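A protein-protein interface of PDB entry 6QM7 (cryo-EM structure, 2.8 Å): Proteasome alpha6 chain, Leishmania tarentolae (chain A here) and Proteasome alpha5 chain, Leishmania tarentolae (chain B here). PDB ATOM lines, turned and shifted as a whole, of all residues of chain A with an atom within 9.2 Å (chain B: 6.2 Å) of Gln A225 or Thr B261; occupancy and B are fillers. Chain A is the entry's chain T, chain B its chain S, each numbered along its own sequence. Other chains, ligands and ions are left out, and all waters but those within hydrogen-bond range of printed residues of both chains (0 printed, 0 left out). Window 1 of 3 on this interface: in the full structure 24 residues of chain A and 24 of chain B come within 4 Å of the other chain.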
ATOM      1  N   SER A 197      17.973 -21.257  -3.170  1.00  0.00           N
ATOM      2  CA  SER A 197      18.233 -20.321  -4.296  1.00  0.00           C
ATOM      3  C   SER A 197      16.962 -19.522  -4.574  1.00  0.00           C
ATOM      4  O   SER A 197      15.866 -20.100  -4.432  1.00  0.00           O
ATOM      5  CB  SER A 197      18.718 -21.033  -5.532  1.00  0.00           C
ATOM      6  OG  SER A 197      17.997 -22.237  -5.734  1.00  0.00           O
ATOM      7  N   ALA A 212      13.108 -18.495 -11.535  1.00  0.00           N
ATOM      8  CA  ALA A 212      14.008 -19.122 -10.542  1.00  0.00           C
ATOM      9  C   ALA A 212      15.448 -18.980 -11.018  1.00  0.00           C
ATOM     10  O   ALA A 212      15.692 -19.255 -12.194  1.00  0.00           O
ATOM     11  CB  ALA A 212      13.639 -20.574 -10.374  1.00  0.00           C
ATOM     12  N   LEU A 213      16.347 -18.574 -10.125  1.00  0.00           N
ATOM     13  CA  LEU A 213      17.807 -18.772 -10.298  1.00  0.00           C
ATOM     14  C   LEU A 213      18.129 -20.261 -10.162  1.00  0.00           C
ATOM     15  O   LEU A 213      17.833 -20.844  -9.099  1.00  0.00           O
ATOM     16  CB  LEU A 213      18.581 -17.976  -9.249  1.00  0.00           C
ATOM     17  CG  LEU A 213      18.915 -16.552  -9.666  1.00  0.00           C
ATOM     18  CD1 LEU A 213      19.509 -15.785  -8.490  1.00  0.00           C
ATOM     19  CD2 LEU A 213      19.852 -16.556 -10.869  1.00  0.00           C
ATOM     20  N   LYS A 214      18.707 -20.841 -11.212  1.00  0.00           N
ATOM     21  CA  LYS A 214      19.478 -22.105 -11.139  1.00  0.00           C
ATOM     22  C   LYS A 214      20.883 -21.777 -10.628  1.00  0.00           C
ATOM     23  O   LYS A 214      21.183 -20.582 -10.415  1.00  0.00           O
ATOM     24  CB  LYS A 214      19.530 -22.779 -12.511  1.00  0.00           C
ATOM     25  CG  LYS A 214      18.181 -23.246 -13.034  1.00  0.00           C
ATOM     26  CD  LYS A 214      18.236 -23.824 -14.429  1.00  0.00           C
ATOM     27  CE  LYS A 214      18.609 -22.788 -15.467  1.00  0.00           C
ATOM     28  NZ  LYS A 214      18.289 -23.241 -16.841  1.00  0.00           N
ATOM     29  N   ARG A 215      21.703 -22.809 -10.432  1.00  0.00           N
ATOM     30  CA  ARG A 215      23.140 -22.679 -10.092  1.00  0.00           C
ATOM     31  C   ARG A 215      23.886 -22.316 -11.386  1.00  0.00           C
ATOM     32  O   ARG A 215      23.594 -22.939 -12.432  1.00  0.00           O
ATOM     33  CB  ARG A 215      23.629 -23.972  -9.432  1.00  0.00           C
ATOM     34  CG  ARG A 215      24.836 -23.800  -8.521  1.00  0.00           C
ATOM     35  CD  ARG A 215      25.367 -25.155  -8.082  1.00  0.00           C
ATOM     36  NE  ARG A 215      26.794 -25.137  -7.771  1.00  0.00           N
ATOM     37  CZ  ARG A 215      27.570 -26.214  -7.623  1.00  0.00           C
ATOM     38  NH1 ARG A 215      27.078 -27.438  -7.757  1.00  0.00           N
ATOM     39  NH2 ARG A 215      28.854 -26.056  -7.342  1.00  0.00           N
ATOM     40  N   SER A 222      28.546 -27.581 -16.092  1.00  0.00           N
ATOM     41  CA  SER A 222      27.111 -27.316 -15.792  1.00  0.00           C
ATOM     42  C   SER A 222      26.589 -28.255 -14.694  1.00  0.00           C
ATOM     43  O   SER A 222      27.053 -29.412 -14.607  1.00  0.00           O
ATOM     44  CB  SER A 222      26.265 -27.424 -17.042  1.00  0.00           C
ATOM     45  OG  SER A 222      25.118 -26.595 -16.955  1.00  0.00           O
ATOM     46  N   SER A 223      25.676 -27.744 -13.871  1.00  0.00           N
ATOM     47  CA  SER A 223      24.756 -28.515 -12.999  1.00  0.00           C
ATOM     48  C   SER A 223      23.328 -28.231 -13.464  1.00  0.00           C
ATOM     49  O   SER A 223      23.062 -27.094 -13.903  1.00  0.00           O
ATOM     50  CB  SER A 223      24.927 -28.158 -11.539  1.00  0.00           C
ATOM     51  OG  SER A 223      26.288 -28.233 -11.147  1.00  0.00           O
ATOM     52  N   TYR A 224      22.450 -29.226 -13.392  1.00  0.00           N
ATOM     53  CA  TYR A 224      20.984 -29.039 -13.477  1.00  0.00           C
ATOM     54  C   TYR A 224      20.351 -29.685 -12.248  1.00  0.00           C
ATOM     55  O   TYR A 224      20.756 -30.793 -11.877  1.00  0.00           O
ATOM     56  CB  TYR A 224      20.407 -29.619 -14.772  1.00  0.00           C
ATOM     57  CG  TYR A 224      18.897 -29.662 -14.796  1.00  0.00           C
ATOM     58  CD1 TYR A 224      18.151 -28.497 -14.927  1.00  0.00           C
ATOM     59  CD2 TYR A 224      18.205 -30.857 -14.648  1.00  0.00           C
ATOM     60  CE1 TYR A 224      16.765 -28.521 -14.931  1.00  0.00           C
ATOM     61  CE2 TYR A 224      16.818 -30.899 -14.652  1.00  0.00           C
ATOM     62  CZ  TYR A 224      16.094 -29.725 -14.791  1.00  0.00           C
ATOM     63  OH  TYR A 224      14.730 -29.750 -14.799  1.00  0.00           O
ATOM     64  N   GLN A 225      19.390 -28.993 -11.642  1.00  0.00           N
ATOM     65  CA  GLN A 225      18.561 -29.506 -10.525  1.00  0.00           C
ATOM     66  C   GLN A 225      17.137 -29.010 -10.754  1.00  0.00           C
ATOM     67  O   GLN A 225      16.964 -27.788 -10.880  1.00  0.00           O
ATOM     68  CB  GLN A 225      19.140 -29.034  -9.193  1.00  0.00           C
ATOM     69  CG  GLN A 225      18.601 -29.787  -7.988  1.00  0.00           C
ATOM     70  CD  GLN A 225      19.567 -29.739  -6.830  1.00  0.00           C
ATOM     71  OE1 GLN A 225      20.248 -28.742  -6.610  1.00  0.00           O
ATOM     72  NE2 GLN A 225      19.634 -30.827  -6.078  1.00  0.00           N
ATOM     73  N   GLU A 226      16.176 -29.931 -10.850  1.00  0.00           N
ATOM     74  CA  GLU A 226      14.752 -29.611 -11.118  1.00  0.00           C
ATOM     75  C   GLU A 226      14.198 -28.875  -9.891  1.00  0.00           C
ATOM     76  O   GLU A 226      13.952 -29.532  -8.859  1.00  0.00           O
ATOM     77  CB  GLU A 226      13.967 -30.884 -11.460  1.00  0.00           C
ATOM     78  CG  GLU A 226      12.604 -30.620 -12.094  1.00  0.00           C
ATOM     79  CD  GLU A 226      11.772 -31.852 -12.418  1.00  0.00           C
ATOM     80  OE1 GLU A 226      12.158 -32.964 -11.990  1.00  0.00           O
ATOM     81  OE2 GLU A 226      10.730 -31.695 -13.086  1.00  0.00           O
ATOM     82  N   LYS A 227      14.079 -27.550 -10.002  1.00  0.00           N
ATOM     83  CA  LYS A 227      13.530 -26.645  -8.961  1.00  0.00           C
ATOM     84  C   LYS A 227      12.107 -26.199  -9.322  1.00  0.00           C
ATOM     85  O   LYS A 227      11.400 -25.781  -8.402  1.00  0.00           O
ATOM     86  CB  LYS A 227      14.405 -25.399  -8.812  1.00  0.00           C
ATOM     87  CG  LYS A 227      15.620 -25.539  -7.901  1.00  0.00           C
ATOM     88  CD  LYS A 227      15.742 -24.416  -6.872  1.00  0.00           C
ATOM     89  CE  LYS A 227      15.594 -23.005  -7.428  1.00  0.00           C
ATOM     90  NZ  LYS A 227      15.194 -22.029  -6.383  1.00  0.00           N
ATOM     91  N   VAL A 228      11.735 -26.216 -10.607  1.00  0.00           N
ATOM     92  CA  VAL A 228      10.383 -25.839 -11.117  1.00  0.00           C
ATOM     93  C   VAL A 228       9.682 -27.096 -11.644  1.00  0.00           C
ATOM     94  O   VAL A 228      10.306 -27.867 -12.384  1.00  0.00           O
ATOM     95  CB  VAL A 228      10.484 -24.739 -12.186  1.00  0.00           C
ATOM     96  CG1 VAL A 228       9.133 -24.415 -12.792  1.00  0.00           C
ATOM     97  CG2 VAL A 228      11.102 -23.471 -11.611  1.00  0.00           C
ATOM     98  N   PHE A 229       8.421 -27.283 -11.273  1.00  0.00           N
ATOM     99  CA  PHE A 229       7.631 -28.513 -11.541  1.00  0.00           C
ATOM    100  C   PHE A 229       6.264 -28.151 -12.105  1.00  0.00           C
ATOM    101  O   PHE A 229       5.540 -27.380 -11.476  1.00  0.00           O
ATOM    102  CB  PHE A 229       7.376 -29.293 -10.251  1.00  0.00           C
ATOM    103  CG  PHE A 229       8.601 -29.814  -9.548  1.00  0.00           C
ATOM    104  CD1 PHE A 229       8.980 -31.141  -9.679  1.00  0.00           C
ATOM    105  CD2 PHE A 229       9.354 -28.990  -8.725  1.00  0.00           C
ATOM    106  CE1 PHE A 229      10.093 -31.629  -9.009  1.00  0.00           C
ATOM    107  CE2 PHE A 229      10.465 -29.480  -8.057  1.00  0.00           C
ATOM    108  CZ  PHE A 229      10.837 -30.797  -8.203  1.00  0.00           C
ATOM    109  N   ILE A 239      10.326 -24.289  -6.071  1.00  0.00           N
ATOM    110  CA  ILE A 239      10.694 -24.609  -4.664  1.00  0.00           C
ATOM    111  C   ILE A 239      11.951 -23.834  -4.280  1.00  0.00           C
ATOM    112  O   ILE A 239      12.697 -23.433  -5.185  1.00  0.00           O
ATOM    113  CB  ILE A 239      10.828 -26.125  -4.482  1.00  0.00           C
ATOM    114  CG1 ILE A 239      12.114 -26.668  -5.104  1.00  0.00           C
ATOM    115  CG2 ILE A 239       9.578 -26.827  -5.016  1.00  0.00           C
ATOM    116  CD1 ILE A 239      12.219 -28.192  -5.068  1.00  0.00           C
ATOM    117  N   GLY A 241      14.784 -24.464  -0.841  1.00  0.00           N
ATOM    118  CA  GLY A 241      15.167 -25.195   0.378  1.00  0.00           C
ATOM    119  C   GLY A 241      15.547 -26.617   0.056  1.00  0.00           C
ATOM    120  O   GLY A 241      16.242 -26.829  -0.954  1.00  0.00           O
ATOM    121  N   LEU A 242      15.086 -27.562   0.869  1.00  0.00           N
ATOM    122  CA  LEU A 242      15.396 -29.002   0.697  1.00  0.00           C
ATOM    123  C   LEU A 242      14.622 -29.505  -0.524  1.00  0.00           C
ATOM    124  O   LEU A 242      13.409 -29.725  -0.435  1.00  0.00           O
ATOM    125  CB  LEU A 242      15.049 -29.763   1.983  1.00  0.00           C
ATOM    126  CG  LEU A 242      15.646 -29.170   3.263  1.00  0.00           C
ATOM    127  CD1 LEU A 242      15.425 -30.104   4.439  1.00  0.00           C
ATOM    128  CD2 LEU A 242      17.134 -28.854   3.089  1.00  0.00           C
ATOM    129  N   VAL A 243      15.336 -29.656  -1.632  1.00  0.00           N
ATOM    130  CA  VAL A 243      14.789 -30.081  -2.948  1.00  0.00           C
ATOM    131  C   VAL A 243      14.117 -31.451  -2.807  1.00  0.00           C
ATOM    132  O   VAL A 243      13.149 -31.705  -3.530  1.00  0.00           O
ATOM    133  CB  VAL A 243      15.908 -30.097  -4.002  1.00  0.00           C
ATOM    134  CG1 VAL A 243      15.411 -30.620  -5.340  1.00  0.00           C
ATOM    135  CG2 VAL A 243      16.545 -28.720  -4.149  1.00  0.00           C
ATOM    136  N   ALA A 244      14.633 -32.306  -1.932  1.00  0.00           N
ATOM    137  CA  ALA A 244      14.055 -33.623  -1.597  1.00  0.00           C
ATOM    138  C   ALA A 244      12.604 -33.460  -1.138  1.00  0.00           C
ATOM    139  O   ALA A 244      11.765 -34.264  -1.554  1.00  0.00           O
ATOM    140  CB  ALA A 244      14.887 -34.268  -0.518  1.00  0.00           C
ATOM    141  N   ASP A 245      12.340 -32.475  -0.280  1.00  0.00           N
ATOM    142  CA  ASP A 245      10.999 -32.191   0.306  1.00  0.00           C
ATOM    143  C   ASP A 245      10.117 -31.533  -0.757  1.00  0.00           C
ATOM    144  O   ASP A 245       8.905 -31.781  -0.745  1.00  0.00           O
ATOM    145  CB  ASP A 245      11.127 -31.329   1.568  1.00  0.00           C
ATOM    146  CG  ASP A 245      11.835 -32.030   2.720  1.00  0.00           C
ATOM    147  OD1 ASP A 245      11.933 -33.283   2.683  1.00  0.00           O
ATOM    148  OD2 ASP A 245      12.289 -31.327   3.651  1.00  0.00           O
ATOM    149  N   GLY A 246      10.709 -30.710  -1.622  1.00  0.00           N
ATOM    150  CA  GLY A 246      10.030 -30.148  -2.801  1.00  0.00           C
ATOM    151  C   GLY A 246       9.432 -31.258  -3.630  1.00  0.00           C
ATOM    152  O   GLY A 246       8.224 -31.218  -3.891  1.00  0.00           O
ATOM    153  N   ARG A 247      10.259 -32.237  -3.981  1.00  0.00           N
ATOM    154  CA  ARG A 247       9.871 -33.446  -4.745  1.00  0.00           C
ATOM    155  C   ARG A 247       8.720 -34.181  -4.062  1.00  0.00           C
ATOM    156  O   ARG A 247       7.861 -34.693  -4.784  1.00  0.00           O
ATOM    157  CB  ARG A 247      11.050 -34.409  -4.870  1.00  0.00           C
ATOM    158  CG  ARG A 247      12.009 -34.081  -6.003  1.00  0.00           C
ATOM    159  CD  ARG A 247      12.823 -35.324  -6.317  1.00  0.00           C
ATOM    160  NE  ARG A 247      11.957 -36.447  -6.695  1.00  0.00           N
ATOM    161  CZ  ARG A 247      12.135 -37.735  -6.357  1.00  0.00           C
ATOM    162  NH1 ARG A 247      13.170 -38.129  -5.622  1.00  0.00           N
ATOM    163  NH2 ARG A 247      11.263 -38.636  -6.781  1.00  0.00           N
ATOM    164  N   LYS A 373      21.222 -19.945 -19.181  1.00  0.00           N
ATOM    165  CA  LYS A 373      21.968 -21.067 -18.554  1.00  0.00           C
ATOM    166  C   LYS A 373      21.808 -21.003 -17.019  1.00  0.00           C
ATOM    167  O   LYS A 373      22.039 -22.062 -16.384  1.00  0.00           O
ATOM    168  CB  LYS A 373      23.413 -21.099 -19.079  1.00  0.00           C
ATOM    169  CG  LYS A 373      24.487 -20.533 -18.159  1.00  0.00           C
ATOM    170  CD  LYS A 373      25.871 -20.475 -18.787  1.00  0.00           C
ATOM    171  CE  LYS A 373      26.046 -19.336 -19.771  1.00  0.00           C
ATOM    172  NZ  LYS A 373      27.479 -19.085 -20.054  1.00  0.00           N
ATOM    173  N   THR A 376      15.605 -20.267 -14.957  1.00  0.00           N
ATOM    174  CA  THR A 376      14.312 -20.841 -15.397  1.00  0.00           C
ATOM    175  C   THR A 376      13.256 -19.733 -15.373  1.00  0.00           C
ATOM    176  O   THR A 376      13.348 -18.843 -14.498  1.00  0.00           O
ATOM    177  CB  THR A 376      13.882 -22.024 -14.516  1.00  0.00           C
ATOM    178  OG1 THR A 376      14.921 -23.006 -14.443  1.00  0.00           O
ATOM    179  CG2 THR A 376      12.624 -22.696 -15.023  1.00  0.00           C
ATOM    180  N   ILE A 388       7.324 -24.448 -18.657  1.00  0.00           N
ATOM    181  CA  ILE A 388       8.683 -24.106 -18.169  1.00  0.00           C
ATOM    182  C   ILE A 388       9.516 -23.813 -19.410  1.00  0.00           C
ATOM    183  O   ILE A 388       9.612 -24.697 -20.274  1.00  0.00           O
ATOM    184  CB  ILE A 388       9.260 -25.257 -17.330  1.00  0.00           C
ATOM    185  CG1 ILE A 388       8.224 -25.791 -16.337  1.00  0.00           C
ATOM    186  CG2 ILE A 388      10.542 -24.829 -16.635  1.00  0.00           C
ATOM    187  CD1 ILE A 388       8.689 -26.988 -15.550  1.00  0.00           C
ATOM    188  N   GLU A 390      13.185 -23.227 -20.714  1.00  0.00           N
ATOM    189  CA  GLU A 390      14.668 -23.288 -20.595  1.00  0.00           C
ATOM    190  C   GLU A 390      15.259 -23.292 -22.013  1.00  0.00           C
ATOM    191  O   GLU A 390      14.602 -23.839 -22.938  1.00  0.00           O
ATOM    192  CB  GLU A 390      15.108 -24.493 -19.752  1.00  0.00           C
ATOM    193  CG  GLU A 390      14.377 -24.609 -18.417  1.00  0.00           C
ATOM    194  CD  GLU A 390      15.099 -25.367 -17.310  1.00  0.00           C
ATOM    195  OE1 GLU A 390      16.198 -24.931 -16.914  1.00  0.00           O
ATOM    196  OE2 GLU A 390      14.554 -26.386 -16.838  1.00  0.00           O
ATOM    197  N   CYS B 217      16.676 -42.277  -5.499  1.00  0.00           N
ATOM    198  CA  CYS B 217      16.470 -41.208  -4.488  1.00  0.00           C
ATOM    199  C   CYS B 217      15.097 -41.296  -3.812  1.00  0.00           C
ATOM    200  O   CYS B 217      14.927 -40.615  -2.792  1.00  0.00           O
ATOM    201  CB  CYS B 217      16.603 -39.849  -5.150  1.00  0.00           C
ATOM    202  SG  CYS B 217      18.244 -39.625  -5.875  1.00  0.00           S
ATOM    203  N   TRP B 254      24.466 -38.216 -13.363  1.00  0.00           N
ATOM    204  CA  TRP B 254      23.681 -37.719 -12.213  1.00  0.00           C
ATOM    205  C   TRP B 254      24.378 -38.096 -10.912  1.00  0.00           C
ATOM    206  O   TRP B 254      25.047 -39.131 -10.897  1.00  0.00           O
ATOM    207  CB  TRP B 254      22.290 -38.320 -12.271  1.00  0.00           C
ATOM    208  CG  TRP B 254      21.483 -37.792 -13.406  1.00  0.00           C
ATOM    209  CD1 TRP B 254      21.544 -38.157 -14.715  1.00  0.00           C
ATOM    210  CD2 TRP B 254      20.473 -36.782 -13.319  1.00  0.00           C
ATOM    211  NE1 TRP B 254      20.623 -37.458 -15.450  1.00  0.00           N
ATOM    212  CE2 TRP B 254      19.958 -36.604 -14.618  1.00  0.00           C
ATOM    213  CE3 TRP B 254      19.964 -36.020 -12.265  1.00  0.00           C
ATOM    214  CZ2 TRP B 254      18.957 -35.686 -14.889  1.00  0.00           C
ATOM    215  CZ3 TRP B 254      18.976 -35.108 -12.535  1.00  0.00           C
ATOM    216  CH2 TRP B 254      18.481 -34.950 -13.829  1.00  0.00           C
ATOM    217  N   GLN B 255      24.205 -37.279  -9.875  1.00  0.00           N
ATOM    218  CA  GLN B 255      24.684 -37.550  -8.501  1.00  0.00           C
ATOM    219  C   GLN B 255      23.476 -37.624  -7.580  1.00  0.00           C
ATOM    220  O   GLN B 255      22.704 -36.668  -7.602  1.00  0.00           O
ATOM    221  CB  GLN B 255      25.610 -36.445  -8.010  1.00  0.00           C
ATOM    222  CG  GLN B 255      26.212 -36.739  -6.646  1.00  0.00           C
ATOM    223  CD  GLN B 255      26.580 -35.482  -5.901  1.00  0.00           C
ATOM    224  OE1 GLN B 255      25.849 -34.491  -5.895  1.00  0.00           O
ATOM    225  NE2 GLN B 255      27.731 -35.510  -5.251  1.00  0.00           N
ATOM    226  N   THR B 256      23.332 -38.708  -6.811  1.00  0.00           N
ATOM    227  CA  THR B 256      22.389 -38.791  -5.664  1.00  0.00           C
ATOM    228  C   THR B 256      23.150 -38.430  -4.391  1.00  0.00           C
ATOM    229  O   THR B 256      24.319 -38.813  -4.281  1.00  0.00           O
ATOM    230  CB  THR B 256      21.694 -40.156  -5.519  1.00  0.00           C
ATOM    231  OG1 THR B 256      22.460 -41.059  -4.719  1.00  0.00           O
ATOM    232  CG2 THR B 256      21.387 -40.804  -6.849  1.00  0.00           C
ATOM    233  N   ASP B 257      22.492 -37.718  -3.480  1.00  0.00           N
ATOM    234  CA  ASP B 257      23.012 -37.403  -2.126  1.00  0.00           C
ATOM    235  C   ASP B 257      22.258 -38.255  -1.112  1.00  0.00           C
ATOM    236  O   ASP B 257      21.318 -38.966  -1.467  1.00  0.00           O
ATOM    237  CB  ASP B 257      22.919 -35.900  -1.819  1.00  0.00           C
ATOM    238  CG  ASP B 257      24.232 -35.133  -1.942  1.00  0.00           C
ATOM    239  OD1 ASP B 257      25.142 -35.602  -2.676  1.00  0.00           O
ATOM    240  OD2 ASP B 257      24.343 -34.071  -1.290  1.00  0.00           O
ATOM    241  N   PRO B 258      22.699 -38.251   0.164  1.00  0.00           N
ATOM    242  CA  PRO B 258      21.929 -38.844   1.257  1.00  0.00           C
ATOM    243  C   PRO B 258      20.564 -38.180   1.485  1.00  0.00           C
ATOM    244  O   PRO B 258      19.643 -38.876   1.882  1.00  0.00           O
ATOM    245  CB  PRO B 258      22.833 -38.590   2.469  1.00  0.00           C
ATOM    246  CG  PRO B 258      24.220 -38.521   1.875  1.00  0.00           C
ATOM    247  CD  PRO B 258      24.002 -37.731   0.609  1.00  0.00           C
ATOM    248  N   SER B 259      20.485 -36.862   1.253  1.00  0.00           N
ATOM    249  CA  SER B 259      19.248 -36.033   1.302  1.00  0.00           C
ATOM    250  C   SER B 259      18.129 -36.672   0.473  1.00  0.00           C
ATOM    251  O   SER B 259      16.966 -36.612   0.924  1.00  0.00           O
ATOM    252  CB  SER B 259      19.512 -34.607   0.855  1.00  0.00           C
ATOM    253  OG  SER B 259      20.654 -34.526   0.014  1.00  0.00           O
ATOM    254  N   GLY B 260      18.467 -37.259  -0.682  1.00  0.00           N
ATOM    255  CA  GLY B 260      17.515 -37.678  -1.728  1.00  0.00           C
ATOM    256  C   GLY B 260      17.461 -36.675  -2.876  1.00  0.00           C
ATOM    257  O   GLY B 260      16.669 -36.897  -3.822  1.00  0.00           O
ATOM    258  N   THR B 261      18.256 -35.597  -2.808  1.00  0.00           N
ATOM    259  CA  THR B 261      18.460 -34.649  -3.935  1.00  0.00           C
ATOM    260  C   THR B 261      19.221 -35.388  -5.031  1.00  0.00           C
ATOM    261  O   THR B 261      20.072 -36.218  -4.695  1.00  0.00           O
ATOM    262  CB  THR B 261      19.246 -33.389  -3.549  1.00  0.00           C
ATOM    263  OG1 THR B 261      20.607 -33.755  -3.328  1.00  0.00           O
ATOM    264  CG2 THR B 261      18.704 -32.682  -2.325  1.00  0.00           C
ATOM    265  N   HIS B 262      18.904 -35.095  -6.283  1.00  0.00           N
ATOM    266  CA  HIS B 262      19.630 -35.604  -7.468  1.00  0.00           C
ATOM    267  C   HIS B 262      19.948 -34.419  -8.372  1.00  0.00           C
ATOM    268  O   HIS B 262      19.055 -33.592  -8.616  1.00  0.00           O
ATOM    269  CB  HIS B 262      18.856 -36.740  -8.154  1.00  0.00           C
ATOM    270  CG  HIS B 262      17.602 -36.327  -8.842  1.00  0.00           C
ATOM    271  ND1 HIS B 262      16.649 -35.543  -8.232  1.00  0.00           N
ATOM    272  CD2 HIS B 262      17.134 -36.611 -10.075  1.00  0.00           C
ATOM    273  CE1 HIS B 262      15.658 -35.335  -9.071  1.00  0.00           C
ATOM    274  NE2 HIS B 262      15.927 -35.990 -10.210  1.00  0.00           N
ATOM    275  N   THR B 263      21.187 -34.362  -8.829  1.00  0.00           N
ATOM    276  CA  THR B 263      21.761 -33.239  -9.593  1.00  0.00           C
ATOM    277  C   THR B 263      22.440 -33.811 -10.832  1.00  0.00           C
ATOM    278  O   THR B 263      23.332 -34.650 -10.674  1.00  0.00           O
ATOM    279  CB  THR B 263      22.760 -32.474  -8.722  1.00  0.00           C
ATOM    280  OG1 THR B 263      22.309 -32.513  -7.366  1.00  0.00           O
ATOM    281  CG2 THR B 263      22.942 -31.045  -9.181  1.00  0.00           C
ATOM    282  N   ARG B 264      22.005 -33.414 -12.019  1.00  0.00           N
ATOM    283  CA  ARG B 264      22.735 -33.739 -13.261  1.00  0.00           C
ATOM    284  C   ARG B 264      24.002 -32.905 -13.249  1.00  0.00           C
ATOM    285  O   ARG B 264      23.920 -31.745 -12.856  1.00  0.00           O
ATOM    286  CB  ARG B 264      21.930 -33.442 -14.524  1.00  0.00           C
ATOM    287  CG  ARG B 264      22.473 -34.168 -15.739  1.00  0.00           C
ATOM    288  CD  ARG B 264      21.627 -33.945 -16.974  1.00  0.00           C
ATOM    289  NE  ARG B 264      21.721 -32.552 -17.382  1.00  0.00           N
ATOM    290  CZ  ARG B 264      20.697 -31.743 -17.610  1.00  0.00           C
ATOM    291  NH1 ARG B 264      19.442 -32.165 -17.505  1.00  0.00           N
ATOM    292  NH2 ARG B 264      20.941 -30.492 -17.958  1.00  0.00           N
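The side-chain hydroxyl of Thr B263 is in hydrogen-bond range of the side-chain amide nitrogen of Gln A225 (3.4 Å). The backbone carbonyl oxygen of Tyr A224 sits at hydrogen-bond distance from the backbone NH of Arg B264 (2.9 Å).
The backbone carbonyl oxygen (O) of Gly B260 lies close to the side-chain sulfur (SG) of Cys B217, at 3.8 Å. The backbone NH of Gln B255 sits at hydrogen-bond distance from the backbone carbonyl oxygen of Thr B263 (2.9 Å). OG of Ser B259 sits at hydrogen-bond distance from OG1 of Thr B261.
Ser A223 touches Arg B264 (CA to O, 3.3 Å). Tyr A224 touches Thr B263 (O to CG2, 3.5 Å). Gln A225 touches Thr B261 (NE2 to CB, 3.6 Å). Gln A225 touches His B262. CB of Ala A244 touches O of Ser B259 (3.4 Å). Cys B217 touches Arg A247 (CB to NH1, 3.9 Å). CE1 of His B262 touches CD of Arg A247, at 3.95 Å.
Of chain B, only Thr B261, His B262 and Thr B263 come within 4 Å of Gln A225. No residue of chain A comes within 4 Å of Gly B260. Printed residues of chain B within 4 Å of Ser A223: Arg B264. Of the printed residues of chain A, Cys B217 touches Arg A247 (3.9 Å). Of the printed residues of chain B, Tyr A224 touches Thr B263 (3.5 Å) and Arg B264 (2.9 Å). Printed residues of chain A within 4 Å of Thr B263: Tyr A224 (3.5 Å) and Gln A225 (3.4 Å). Of the printed residues of chain B, Arg A247 touches Cys B217 (3.9 Å) and His B262 (3.95 Å). Lys A227 touches none of the printed residues of chain B. Ser A222 touches none of the printed residues of chain B. The nearest residue of chain B that does not touch Gln A225 is Arg B264 (5.2 Å). The nearest residue of chain A that does not touch Thr B261 is Ala A244 (4.1 Å). The nearest printed residue of chain A that does not touch Cys B217 is Ala A244 (6.7 Å).
Of the 12 printed residues of chain B, 6 touch a printed residue of chain A. Printed residues of chain B that touch a printed residue of chain A: Cys B217, Ser B259, Thr B261, His B262, Thr B263 and Arg B264. Printed residues of chain A that touch a printed residue of chain B: Ser A223, Tyr A224, Gln A225, Ala A244 and Arg A247. Hydrophobic or aromatic side chains of chain A that line the printed part of chain B: Tyr A224 and Ala A244. Among the printed residues, 9 pairs touch across the chains. Among the printed residues, no Asp or Glu carboxylate lies within 4 Å of a Lys or Arg side-chain nitrogen of the other chain.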
